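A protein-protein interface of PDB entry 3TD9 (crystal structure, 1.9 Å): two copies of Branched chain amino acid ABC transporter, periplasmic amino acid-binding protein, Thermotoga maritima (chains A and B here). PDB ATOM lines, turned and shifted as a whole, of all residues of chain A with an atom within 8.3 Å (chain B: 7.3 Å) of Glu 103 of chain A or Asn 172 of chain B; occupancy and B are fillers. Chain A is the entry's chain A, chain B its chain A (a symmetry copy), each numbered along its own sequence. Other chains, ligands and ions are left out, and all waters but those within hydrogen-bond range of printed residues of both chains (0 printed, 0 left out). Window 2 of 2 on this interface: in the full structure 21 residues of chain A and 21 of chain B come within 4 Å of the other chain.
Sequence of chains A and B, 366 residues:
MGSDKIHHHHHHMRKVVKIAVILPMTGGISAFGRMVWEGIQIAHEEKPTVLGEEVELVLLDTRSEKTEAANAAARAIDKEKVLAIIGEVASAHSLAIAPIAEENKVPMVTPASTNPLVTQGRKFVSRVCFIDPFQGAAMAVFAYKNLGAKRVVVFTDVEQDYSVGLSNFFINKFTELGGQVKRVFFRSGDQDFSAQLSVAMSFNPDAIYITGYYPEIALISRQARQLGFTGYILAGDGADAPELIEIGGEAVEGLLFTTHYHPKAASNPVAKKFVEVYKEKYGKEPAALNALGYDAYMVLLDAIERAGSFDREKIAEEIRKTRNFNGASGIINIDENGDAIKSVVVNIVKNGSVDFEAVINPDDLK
NH2 of Arg 183 of chain B lies within salt-bridge range of OE2 of Glu 103 of chain A (2.7 Å).
The side-chain amide nitrogen (ND2) of Asn 104 of chain A sits at hydrogen-bond distance from the backbone carbonyl oxygen (O) of Ile 100 of chain A, 2.7 Å away. The side-chain amide oxygen (OD1) of Asn 168 of chain B sits close to the backbone carbonyl oxygen (O) of Val 164 of chain B (2.9 Å). ND2 of Asn 172 of chain B lies close to O of Asn 168 of chain B, at 3.4 Å. The guanidinium group of Arg 183 of chain B sits at hydrogen-bond distance from the side-chain amide oxygen of Asn 168 of chain B, 2.8 Å away. The side-chain hydroxyl of Thr 175 of chain B is in hydrogen-bond range of the backbone carbonyl oxygen of Ile 171 of chain B, 2.8 Å away. O of Asn 172 of chain B lies within hydrogen-bond range of OG1 of Thr 175 of chain B (3.4 Å).
Pro 99 of chain A touches Asn 168 of chain B. CB of Pro 99 of chain A touches NH2 of Arg 183 of chain B, 3.98 Å away. Ile 100 of chain A touches Arg 183 of chain B (CG1 to NE, 3.9 Å). Glu 103 of chain A touches Asn 168 of chain B (OE2 to CA, 3.9 Å). CD of Glu 103 of chain A touches CG2 of Ile 171 of chain B, at 3.5 Å. Asn 172 of chain B touches Glu 103 of chain A. Asn 168 of chain B touches Arg 122 of chain A (ND2 to NH2, 3.98 Å).
Printed residues of chain B within 4 Å of Pro 99 of chain A: Asn 168 and Arg 183. Of the printed residues of chain B, Ile 100 of chain A touches Arg 183 (3.9 Å). Of the printed residues of chain B, Glu 103 of chain A touches Asn 168, Ile 171, Asn 172 and Arg 183. Printed residues of chain B within 4 Å of Arg 122 of chain A: Asn 168 (3.98 Å). Of the printed residues of chain A, Asn 168 of chain B touches Pro 99 (3.2 Å), Glu 103 (3.9 Å) and Arg 122 (3.98 Å). Of the printed residues of chain A, Ile 171 of chain B touches Glu 103. Printed residues of chain A within 4 Å of Asn 172 of chain B: Glu 103. The nearest printed residue of chain B that does not touch Glu 103 of chain A is Ser 167 of chain B (4.8 Å). The nearest printed residue of chain A that does not touch Asn 172 of chain B is Glu 102 of chain A (5.5 Å). The nearest printed residue of chain B that does not touch Pro 99 of chain A is Val 164 of chain B (5.2 Å).
Of the 19 printed residues of chain B, 4 touch a printed residue of chain A. Hydrophobic or aromatic side chains of chain B within 4 Å of the printed part of chain A: Ile 171. Of the 17 printed residues of chain A, 4 touch a printed residue of chain B. Among the printed residues, 8 pairs touch across the chains.
No position is printed for both chains. Of the 8 pairs that touch across the chains among the printed residues, none has its exchanged pair printed and touching as well.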
ATOM      1  N   ILE A  77      -2.002  19.164   2.265  1.00  0.00           N
ATOM      2  CA  ILE A  77      -1.444  19.539   3.547  1.00  0.00           C
ATOM      3  C   ILE A  77      -0.797  18.341   4.232  1.00  0.00           C
ATOM      4  O   ILE A  77       0.355  18.432   4.612  1.00  0.00           O
ATOM      5  CB  ILE A  77      -2.488  20.228   4.430  1.00  0.00           C
ATOM      6  CG1 ILE A  77      -2.919  21.544   3.736  1.00  0.00           C
ATOM      7  CG2 ILE A  77      -1.889  20.483   5.828  1.00  0.00           C
ATOM      8  CD1 ILE A  77      -4.158  22.202   4.281  1.00  0.00           C
ATOM      9  N   ALA A  96     -15.154  24.235   1.363  1.00  0.00           N
ATOM     10  CA  ALA A  96     -14.781  22.901   1.841  1.00  0.00           C
ATOM     11  C   ALA A  96     -13.332  22.911   2.261  1.00  0.00           C
ATOM     12  O   ALA A  96     -12.947  22.268   3.261  1.00  0.00           O
ATOM     13  CB  ALA A  96     -15.012  21.855   0.767  1.00  0.00           C
ATOM     14  N   ILE A  97     -12.508  23.676   1.549  1.00  0.00           N
ATOM     15  CA  ILE A  97     -11.076  23.623   1.834  1.00  0.00           C
ATOM     16  C   ILE A  97     -10.509  24.724   2.716  1.00  0.00           C
ATOM     17  O   ILE A  97      -9.483  24.500   3.383  1.00  0.00           O
ATOM     18  CB  ILE A  97     -10.230  23.473   0.540  1.00  0.00           C
ATOM     19  CG1 ILE A  97     -10.202  24.726  -0.278  1.00  0.00           C
ATOM     20  CG2 ILE A  97     -10.750  22.299  -0.300  1.00  0.00           C
ATOM     21  CD1 ILE A  97      -9.528  24.509  -1.665  1.00  0.00           C
ATOM     22  N   ALA A  98     -11.142  25.898   2.730  1.00  0.00           N
ATOM     23  CA  ALA A  98     -10.678  27.032   3.579  1.00  0.00           C
ATOM     24  C   ALA A  98     -10.480  26.620   5.044  1.00  0.00           C
ATOM     25  O   ALA A  98      -9.488  26.956   5.636  1.00  0.00           O
ATOM     26  CB  ALA A  98     -11.626  28.218   3.499  1.00  0.00           C
ATOM     27  N   PRO A  99     -11.403  25.834   5.622  1.00  0.00           N
ATOM     28  CA  PRO A  99     -11.110  25.479   7.023  1.00  0.00           C
ATOM     29  C   PRO A  99      -9.878  24.611   7.169  1.00  0.00           C
ATOM     30  O   PRO A  99      -9.174  24.718   8.174  1.00  0.00           O
ATOM     31  CB  PRO A  99     -12.378  24.743   7.493  1.00  0.00           C
ATOM     32  CG  PRO A  99     -13.116  24.382   6.249  1.00  0.00           C
ATOM     33  CD  PRO A  99     -12.733  25.359   5.197  1.00  0.00           C
ATOM     34  N   ILE A 100      -9.605  23.772   6.170  1.00  0.00           N
ATOM     35  CA  ILE A 100      -8.442  22.901   6.208  1.00  0.00           C
ATOM     36  C   ILE A 100      -7.129  23.699   6.144  1.00  0.00           C
ATOM     37  O   ILE A 100      -6.136  23.375   6.830  1.00  0.00           O
ATOM     38  CB  ILE A 100      -8.510  21.823   5.087  1.00  0.00           C
ATOM     39  CG1 ILE A 100      -9.810  20.995   5.189  1.00  0.00           C
ATOM     40  CG2 ILE A 100      -7.350  20.806   5.202  1.00  0.00           C
ATOM     41  CD1 ILE A 100      -9.951  19.962   4.079  1.00  0.00           C
ATOM     42  N   ALA A 101      -7.123  24.715   5.287  1.00  0.00           N
ATOM     43  CA  ALA A 101      -6.004  25.631   5.141  1.00  0.00           C
ATOM     44  C   ALA A 101      -5.809  26.371   6.464  1.00  0.00           C
ATOM     45  O   ALA A 101      -4.692  26.420   6.971  1.00  0.00           O
ATOM     46  CB  ALA A 101      -6.252  26.637   3.980  1.00  0.00           C
ATOM     47  N   GLU A 102      -6.881  26.901   7.033  1.00  0.00           N
ATOM     48  CA  GLU A 102      -6.790  27.706   8.267  1.00  0.00           C
ATOM     49  C   GLU A 102      -6.289  26.904   9.454  1.00  0.00           C
ATOM     50  O   GLU A 102      -5.434  27.365  10.194  1.00  0.00           O
ATOM     51  CB  GLU A 102      -8.155  28.315   8.618  1.00  0.00           C
ATOM     52  CG  GLU A 102      -8.179  29.314   9.767  1.00  0.00           C
ATOM     53  CD  GLU A 102      -7.569  30.667   9.415  1.00  0.00           C
ATOM     54  OE1 GLU A 102      -7.234  30.904   8.231  1.00  0.00           O
ATOM     55  OE2 GLU A 102      -7.437  31.499  10.337  1.00  0.00           O
ATOM     56  N   GLU A 103      -6.837  25.701   9.633  1.00  0.00           N
ATOM     57  CA  GLU A 103      -6.487  24.828  10.764  1.00  0.00           C
ATOM     58  C   GLU A 103      -5.021  24.487  10.738  1.00  0.00           C
ATOM     59  O   GLU A 103      -4.401  24.282  11.772  1.00  0.00           O
ATOM     60  CB  GLU A 103      -7.287  23.502  10.677  1.00  0.00           C
ATOM     61  CG  GLU A 103      -8.784  23.651  10.955  1.00  0.00           C
ATOM     62  CD  GLU A 103      -9.677  22.551  10.297  1.00  0.00           C
ATOM     63  OE1 GLU A 103      -9.167  21.524   9.763  1.00  0.00           O
ATOM     64  OE2 GLU A 103     -10.909  22.723  10.354  1.00  0.00           O
ATOM     65  N   ASN A 104      -4.472  24.370   9.536  1.00  0.00           N
ATOM     66  CA  ASN A 104      -3.080  24.012   9.357  1.00  0.00           C
ATOM     67  C   ASN A 104      -2.167  25.202   9.028  1.00  0.00           C
ATOM     68  O   ASN A 104      -0.993  25.013   8.744  1.00  0.00           O
ATOM     69  CB  ASN A 104      -2.968  22.899   8.307  1.00  0.00           C
ATOM     70  CG  ASN A 104      -3.675  21.656   8.746  1.00  0.00           C
ATOM     71  OD1 ASN A 104      -3.148  20.942   9.593  1.00  0.00           O
ATOM     72  ND2 ASN A 104      -4.921  21.442   8.277  1.00  0.00           N
ATOM     73  N   LYS A 105      -2.685  26.418   9.139  1.00  0.00           N
ATOM     74  CA  LYS A 105      -1.884  27.644   8.894  1.00  0.00           C
ATOM     75  C   LYS A 105      -1.171  27.610   7.556  1.00  0.00           C
ATOM     76  O   LYS A 105       0.033  27.857   7.460  1.00  0.00           O
ATOM     77  CB  LYS A 105      -0.848  27.809   9.998  1.00  0.00           C
ATOM     78  CG  LYS A 105      -1.423  28.029  11.375  1.00  0.00           C
ATOM     79  CD  LYS A 105      -0.255  28.143  12.369  1.00  0.00           C
ATOM     80  CE  LYS A 105      -0.625  28.968  13.567  1.00  0.00           C
ATOM     81  NZ  LYS A 105      -1.876  28.468  14.188  1.00  0.00           N
ATOM     82  N   VAL A 106      -1.910  27.260   6.514  1.00  0.00           N
ATOM     83  CA  VAL A 106      -1.357  27.194   5.186  1.00  0.00           C
ATOM     84  C   VAL A 106      -2.035  28.314   4.399  1.00  0.00           C
ATOM     85  O   VAL A 106      -3.259  28.332   4.266  1.00  0.00           O
ATOM     86  CB  VAL A 106      -1.637  25.828   4.516  1.00  0.00           C
ATOM     87  CG1 VAL A 106      -1.291  25.889   3.026  1.00  0.00           C
ATOM     88  CG2 VAL A 106      -0.862  24.713   5.206  1.00  0.00           C
ATOM     89  N   GLY A 121     -13.593  35.570   9.239  1.00  0.00           N
ATOM     90  CA  GLY A 121     -13.139  34.959  10.486  1.00  0.00           C
ATOM     91  C   GLY A 121     -11.853  34.148  10.345  1.00  0.00           C
ATOM     92  O   GLY A 121     -11.507  33.420  11.244  1.00  0.00           O
ATOM     93  N   ARG A 122     -11.160  34.243   9.205  1.00  0.00           N
ATOM     94  CA  ARG A 122      -9.937  33.473   8.966  1.00  0.00           C
ATOM     95  C   ARG A 122      -8.769  34.430   8.756  1.00  0.00           C
ATOM     96  O   ARG A 122      -8.980  35.557   8.339  1.00  0.00           O
ATOM     97  CB  ARG A 122     -10.110  32.602   7.716  1.00  0.00           C
ATOM     98  CG  ARG A 122     -11.222  31.580   7.864  1.00  0.00           C
ATOM     99  CD  ARG A 122     -11.117  30.416   6.864  1.00  0.00           C
ATOM    100  NE  ARG A 122     -12.003  29.351   7.330  1.00  0.00           N
ATOM    101  CZ  ARG A 122     -13.256  29.144   6.922  1.00  0.00           C
ATOM    102  NH1 ARG A 122     -13.823  29.872   5.957  1.00  0.00           N
ATOM    103  NH2 ARG A 122     -13.946  28.184   7.487  1.00  0.00           N
ATOM    104  N   PHE A 124      -5.676  33.056   7.223  1.00  0.00           N
ATOM    105  CA  PHE A 124      -4.801  32.468   6.216  1.00  0.00           C
ATOM    106  C   PHE A 124      -5.407  32.403   4.805  1.00  0.00           C
ATOM    107  O   PHE A 124      -4.728  32.024   3.866  1.00  0.00           O
ATOM    108  CB  PHE A 124      -4.330  31.078   6.677  1.00  0.00           C
ATOM    109  CG  PHE A 124      -3.301  31.129   7.777  1.00  0.00           C
ATOM    110  CD1 PHE A 124      -3.691  31.234   9.097  1.00  0.00           C
ATOM    111  CD2 PHE A 124      -1.945  31.090   7.480  1.00  0.00           C
ATOM    112  CE1 PHE A 124      -2.742  31.331  10.124  1.00  0.00           C
ATOM    113  CE2 PHE A 124      -0.993  31.186   8.487  1.00  0.00           C
ATOM    114  CZ  PHE A 124      -1.408  31.296   9.829  1.00  0.00           C
ATOM    115  N   VAL A 125      -6.664  32.793   4.654  1.00  0.00           N
ATOM    116  CA  VAL A 125      -7.420  32.585   3.421  1.00  0.00           C
ATOM    117  C   VAL A 125      -7.834  33.935   2.859  1.00  0.00           C
ATOM    118  O   VAL A 125      -8.451  34.742   3.545  1.00  0.00           O
ATOM    119  CB  VAL A 125      -8.671  31.708   3.696  1.00  0.00           C
ATOM    120  CG1 VAL A 125      -9.397  31.428   2.406  1.00  0.00           C
ATOM    121  CG2 VAL A 125      -8.242  30.385   4.344  1.00  0.00           C
ATOM    122  N   ARG A 312       5.095  30.781   6.851  1.00  0.00           N
ATOM    123  CA  ARG A 312       3.700  30.828   6.479  1.00  0.00           C
ATOM    124  C   ARG A 312       2.868  31.911   7.162  1.00  0.00           C
ATOM    125  O   ARG A 312       1.963  32.482   6.526  1.00  0.00           O
ATOM    126  CB  ARG A 312       3.091  29.442   6.674  1.00  0.00           C
ATOM    127  CG  ARG A 312       3.554  28.500   5.564  1.00  0.00           C
ATOM    128  CD  ARG A 312       2.844  27.194   5.554  1.00  0.00           C
ATOM    129  NE  ARG A 312       3.593  26.212   6.282  1.00  0.00           N
ATOM    130  CZ  ARG A 312       3.341  25.793   7.517  1.00  0.00           C
ATOM    131  NH1 ARG A 312       2.320  26.253   8.229  1.00  0.00           N
ATOM    132  NH2 ARG A 312       4.141  24.883   8.038  1.00  0.00           N
ATOM    133  N   ALA B 137     -16.676  23.065  20.516  1.00  0.00           N
ATOM    134  CA  ALA B 137     -15.680  23.285  21.549  1.00  0.00           C
ATOM    135  C   ALA B 137     -15.943  22.378  22.747  1.00  0.00           C
ATOM    136  O   ALA B 137     -14.988  21.834  23.358  1.00  0.00           O
ATOM    137  CB  ALA B 137     -15.652  24.786  21.952  1.00  0.00           C
ATOM    138  N   ALA B 140     -14.794  18.892  22.043  1.00  0.00           N
ATOM    139  CA  ALA B 140     -13.344  18.933  21.923  1.00  0.00           C
ATOM    140  C   ALA B 140     -12.698  18.853  23.316  1.00  0.00           C
ATOM    141  O   ALA B 140     -11.785  18.070  23.519  1.00  0.00           O
ATOM    142  CB  ALA B 140     -12.871  20.191  21.177  1.00  0.00           C
ATOM    143  N   VAL B 164     -20.255  20.586   8.180  1.00  0.00           N
ATOM    144  CA  VAL B 164     -19.061  21.261   7.793  1.00  0.00           C
ATOM    145  C   VAL B 164     -18.634  22.257   8.898  1.00  0.00           C
ATOM    146  O   VAL B 164     -17.449  22.328   9.283  1.00  0.00           O
ATOM    147  CB  VAL B 164     -19.261  21.966   6.453  1.00  0.00           C
ATOM    148  CG1 VAL B 164     -18.085  22.838   6.151  1.00  0.00           C
ATOM    149  CG2 VAL B 164     -19.516  20.909   5.301  1.00  0.00           C
ATOM    150  N   GLY B 165     -19.609  22.974   9.436  1.00  0.00           N
ATOM    151  CA  GLY B 165     -19.379  23.941  10.477  1.00  0.00           C
ATOM    152  C   GLY B 165     -18.951  23.321  11.782  1.00  0.00           C
ATOM    153  O   GLY B 165     -17.983  23.753  12.336  1.00  0.00           O
ATOM    154  N   LEU B 166     -19.669  22.315  12.263  1.00  0.00           N
ATOM    155  CA  LEU B 166     -19.367  21.693  13.538  1.00  0.00           C
ATOM    156  C   LEU B 166     -17.976  21.049  13.546  1.00  0.00           C
ATOM    157  O   LEU B 166     -17.251  21.092  14.564  1.00  0.00           O
ATOM    158  CB  LEU B 166     -20.403  20.628  13.885  1.00  0.00           C
ATOM    159  CG  LEU B 166     -20.346  19.928  15.270  1.00  0.00           C
ATOM    160  CD1 LEU B 166     -20.331  20.946  16.456  1.00  0.00           C
ATOM    161  CD2 LEU B 166     -21.533  18.965  15.425  1.00  0.00           C
ATOM    162  N   SER B 167     -17.641  20.391  12.438  1.00  0.00           N
ATOM    163  CA  SER B 167     -16.329  19.786  12.287  1.00  0.00           C
ATOM    164  C   SER B 167     -15.254  20.885  12.437  1.00  0.00           C
ATOM    165  O   SER B 167     -14.264  20.677  13.170  1.00  0.00           O
ATOM    166  CB  SER B 167     -16.156  19.130  10.900  1.00  0.00           C
ATOM    167  OG  SER B 167     -16.840  17.896  10.757  1.00  0.00           O
ATOM    168  N   ASN B 168     -15.393  22.014  11.721  1.00  0.00           N
ATOM    169  CA  ASN B 168     -14.473  23.141  11.817  1.00  0.00           C
ATOM    170  C   ASN B 168     -14.343  23.588  13.284  1.00  0.00           C
ATOM    171  O   ASN B 168     -13.267  23.823  13.791  1.00  0.00           O
ATOM    172  CB  ASN B 168     -14.959  24.352  10.961  1.00  0.00           C
ATOM    173  CG  ASN B 168     -15.109  24.034   9.452  1.00  0.00           C
ATOM    174  OD1 ASN B 168     -14.603  23.015   8.967  1.00  0.00           O
ATOM    175  ND2 ASN B 168     -15.849  24.912   8.708  1.00  0.00           N
ATOM    176  N   PHE B 169     -15.481  23.742  13.947  1.00  0.00           N
ATOM    177  CA  PHE B 169     -15.429  24.287  15.340  1.00  0.00           C
ATOM    178  C   PHE B 169     -14.820  23.304  16.315  1.00  0.00           C
ATOM    179  O   PHE B 169     -14.046  23.691  17.192  1.00  0.00           O
ATOM    180  CB  PHE B 169     -16.785  24.786  15.836  1.00  0.00           C
ATOM    181  CG  PHE B 169     -17.321  25.960  15.051  1.00  0.00           C
ATOM    182  CD1 PHE B 169     -16.596  27.137  14.955  1.00  0.00           C
ATOM    183  CD2 PHE B 169     -18.551  25.881  14.424  1.00  0.00           C
ATOM    184  CE1 PHE B 169     -17.078  28.238  14.195  1.00  0.00           C
ATOM    185  CE2 PHE B 169     -19.046  26.974  13.680  1.00  0.00           C
ATOM    186  CZ  PHE B 169     -18.305  28.138  13.559  1.00  0.00           C
ATOM    187  N   PHE B 170     -15.123  22.022  16.142  1.00  0.00           N
ATOM    188  CA  PHE B 170     -14.481  20.995  16.956  1.00  0.00           C
ATOM    189  C   PHE B 170     -12.962  20.997  16.737  1.00  0.00           C
ATOM    190  O   PHE B 170     -12.177  21.019  17.679  1.00  0.00           O
ATOM    191  CB  PHE B 170     -15.037  19.625  16.619  1.00  0.00           C
ATOM    192  CG  PHE B 170     -14.301  18.497  17.283  1.00  0.00           C
ATOM    193  CD1 PHE B 170     -14.677  18.059  18.568  1.00  0.00           C
ATOM    194  CD2 PHE B 170     -13.211  17.896  16.648  1.00  0.00           C
ATOM    195  CE1 PHE B 170     -14.009  16.998  19.164  1.00  0.00           C
ATOM    196  CE2 PHE B 170     -12.525  16.850  17.255  1.00  0.00           C
ATOM    197  CZ  PHE B 170     -12.922  16.396  18.514  1.00  0.00           C
ATOM    198  N   ILE B 171     -12.552  21.000  15.487  1.00  0.00           N
ATOM    199  CA  ILE B 171     -11.135  20.876  15.141  1.00  0.00           C
ATOM    200  C   ILE B 171     -10.329  22.074  15.642  1.00  0.00           C
ATOM    201  O   ILE B 171      -9.229  21.897  16.168  1.00  0.00           O
ATOM    202  CB  ILE B 171     -10.953  20.604  13.638  1.00  0.00           C
ATOM    203  CG1 ILE B 171     -11.540  19.227  13.274  1.00  0.00           C
ATOM    204  CG2 ILE B 171      -9.472  20.627  13.250  1.00  0.00           C
ATOM    205  CD1 ILE B 171     -11.726  18.981  11.761  1.00  0.00           C
ATOM    206  N   ASN B 172     -10.861  23.286  15.507  1.00  0.00           N
ATOM    207  CA  ASN B 172     -10.180  24.471  16.017  1.00  0.00           C
ATOM    208  C   ASN B 172      -9.853  24.296  17.510  1.00  0.00           C
ATOM    209  O   ASN B 172      -8.721  24.505  17.946  1.00  0.00           O
ATOM    210  CB  ASN B 172     -11.049  25.720  15.850  1.00  0.00           C
ATOM    211  CG  ASN B 172     -11.125  26.209  14.408  1.00  0.00           C
ATOM    212  OD1 ASN B 172     -10.270  25.882  13.578  1.00  0.00           O
ATOM    213  ND2 ASN B 172     -12.152  27.026  14.114  1.00  0.00           N
ATOM    214  N   LYS B 173     -10.853  23.926  18.293  1.00  0.00           N
ATOM    215  CA  LYS B 173     -10.644  23.758  19.732  1.00  0.00           C
ATOM    216  C   LYS B 173      -9.768  22.522  20.073  1.00  0.00           C
ATOM    217  O   LYS B 173      -8.891  22.608  20.916  1.00  0.00           O
ATOM    218  CB  LYS B 173     -11.979  23.686  20.464  1.00  0.00           C
ATOM    219  CG  LYS B 173     -11.856  23.616  22.015  1.00  0.00           C
ATOM    220  CD  LYS B 173     -11.529  24.991  22.587  1.00  0.00           C
ATOM    221  CE  LYS B 173     -11.449  24.958  24.081  1.00  0.00           C
ATOM    222  NZ  LYS B 173     -11.067  26.282  24.610  1.00  0.00           N
ATOM    223  N   PHE B 174     -10.024  21.379  19.445  1.00  0.00           N
ATOM    224  CA  PHE B 174      -9.285  20.151  19.756  1.00  0.00           C
ATOM    225  C   PHE B 174      -7.774  20.300  19.522  1.00  0.00           C
ATOM    226  O   PHE B 174      -6.942  19.887  20.364  1.00  0.00           O
ATOM    227  CB  PHE B 174      -9.814  18.962  18.946  1.00  0.00           C
ATOM    228  CG  PHE B 174      -9.298  17.641  19.426  1.00  0.00           C
ATOM    229  CD1 PHE B 174      -9.676  17.160  20.660  1.00  0.00           C
ATOM    230  CD2 PHE B 174      -8.427  16.887  18.660  1.00  0.00           C
ATOM    231  CE1 PHE B 174      -9.228  15.920  21.124  1.00  0.00           C
ATOM    232  CE2 PHE B 174      -7.954  15.645  19.121  1.00  0.00           C
ATOM    233  CZ  PHE B 174      -8.346  15.166  20.359  1.00  0.00           C
ATOM    234  N   THR B 175      -7.423  20.911  18.401  1.00  0.00           N
ATOM    235  CA  THR B 175      -6.027  21.171  18.056  1.00  0.00           C
ATOM    236  C   THR B 175      -5.417  22.294  18.900  1.00  0.00           C
ATOM    237  O   THR B 175      -4.244  22.192  19.251  1.00  0.00           O
ATOM    238  CB  THR B 175      -5.814  21.442  16.553  1.00  0.00           C
ATOM    239  OG1 THR B 175      -6.522  22.607  16.154  1.00  0.00           O
ATOM    240  CG2 THR B 175      -6.263  20.227  15.680  1.00  0.00           C
ATOM    241  N   GLU B 176      -6.203  23.314  19.269  1.00  0.00           N
ATOM    242  CA  GLU B 176      -5.758  24.353  20.213  1.00  0.00           C
ATOM    243  C   GLU B 176      -5.358  23.729  21.557  1.00  0.00           C
ATOM    244  O   GLU B 176      -4.445  24.199  22.209  1.00  0.00           O
ATOM    245  CB  GLU B 176      -6.847  25.424  20.430  1.00  0.00           C
ATOM    246  CG  GLU B 176      -6.591  26.476  21.510  1.00  0.00           C
ATOM    247  CD  GLU B 176      -7.895  27.078  22.089  1.00  0.00           C
ATOM    248  OE1 GLU B 176      -8.595  27.828  21.354  1.00  0.00           O
ATOM    249  OE2 GLU B 176      -8.227  26.786  23.270  1.00  0.00           O
ATOM    250  N   LEU B 177      -6.045  22.678  21.950  1.00  0.00           N
ATOM    251  CA  LEU B 177      -5.720  21.943  23.151  1.00  0.00           C
ATOM    252  C   LEU B 177      -4.462  21.074  23.003  1.00  0.00           C
ATOM    253  O   LEU B 177      -3.924  20.632  23.999  1.00  0.00           O
ATOM    254  CB  LEU B 177      -6.907  21.068  23.567  1.00  0.00           C
ATOM    255  CG  LEU B 177      -8.161  21.815  24.059  1.00  0.00           C
ATOM    256  CD1 LEU B 177      -9.242  20.833  24.315  1.00  0.00           C
ATOM    257  CD2 LEU B 177      -7.904  22.660  25.320  1.00  0.00           C
ATOM    258  N   GLY B 178      -4.017  20.824  21.768  1.00  0.00           N
ATOM    259  CA  GLY B 178      -2.838  20.002  21.501  1.00  0.00           C
ATOM    260  C   GLY B 178      -3.122  18.662  20.823  1.00  0.00           C
ATOM    261  O   GLY B 178      -2.206  17.861  20.604  1.00  0.00           O
ATOM    262  N   VAL B 181      -5.617  15.688  14.468  1.00  0.00           N
ATOM    263  CA  VAL B 181      -6.788  15.302  13.725  1.00  0.00           C
ATOM    264  C   VAL B 181      -6.463  14.869  12.297  1.00  0.00           C
ATOM    265  O   VAL B 181      -5.562  15.405  11.654  1.00  0.00           O
ATOM    266  CB  VAL B 181      -7.819  16.474  13.702  1.00  0.00           C
ATOM    267  CG1 VAL B 181      -8.849  16.289  12.597  1.00  0.00           C
ATOM    268  CG2 VAL B 181      -8.443  16.662  15.126  1.00  0.00           C
ATOM    269  N   ARG B 183      -8.907  14.296   8.790  1.00  0.00           N
ATOM    270  CA  ARG B 183     -10.230  14.556   8.245  1.00  0.00           C
ATOM    271  C   ARG B 183     -10.567  13.587   7.100  1.00  0.00           C
ATOM    272  O   ARG B 183      -9.742  13.318   6.217  1.00  0.00           O
ATOM    273  CB  ARG B 183     -10.281  15.984   7.697  1.00  0.00           C
ATOM    274  CG  ARG B 183     -10.446  17.078   8.730  1.00  0.00           C
ATOM    275  CD  ARG B 183     -10.276  18.371   8.009  1.00  0.00           C
ATOM    276  NE  ARG B 183     -10.863  19.566   8.610  1.00  0.00           N
ATOM    277  CZ  ARG B 183     -12.150  19.909   8.551  1.00  0.00           C
ATOM    278  NH1 ARG B 183     -13.073  19.088   8.034  1.00  0.00           N
ATOM    279  NH2 ARG B 183     -12.528  21.072   9.025  1.00  0.00           N
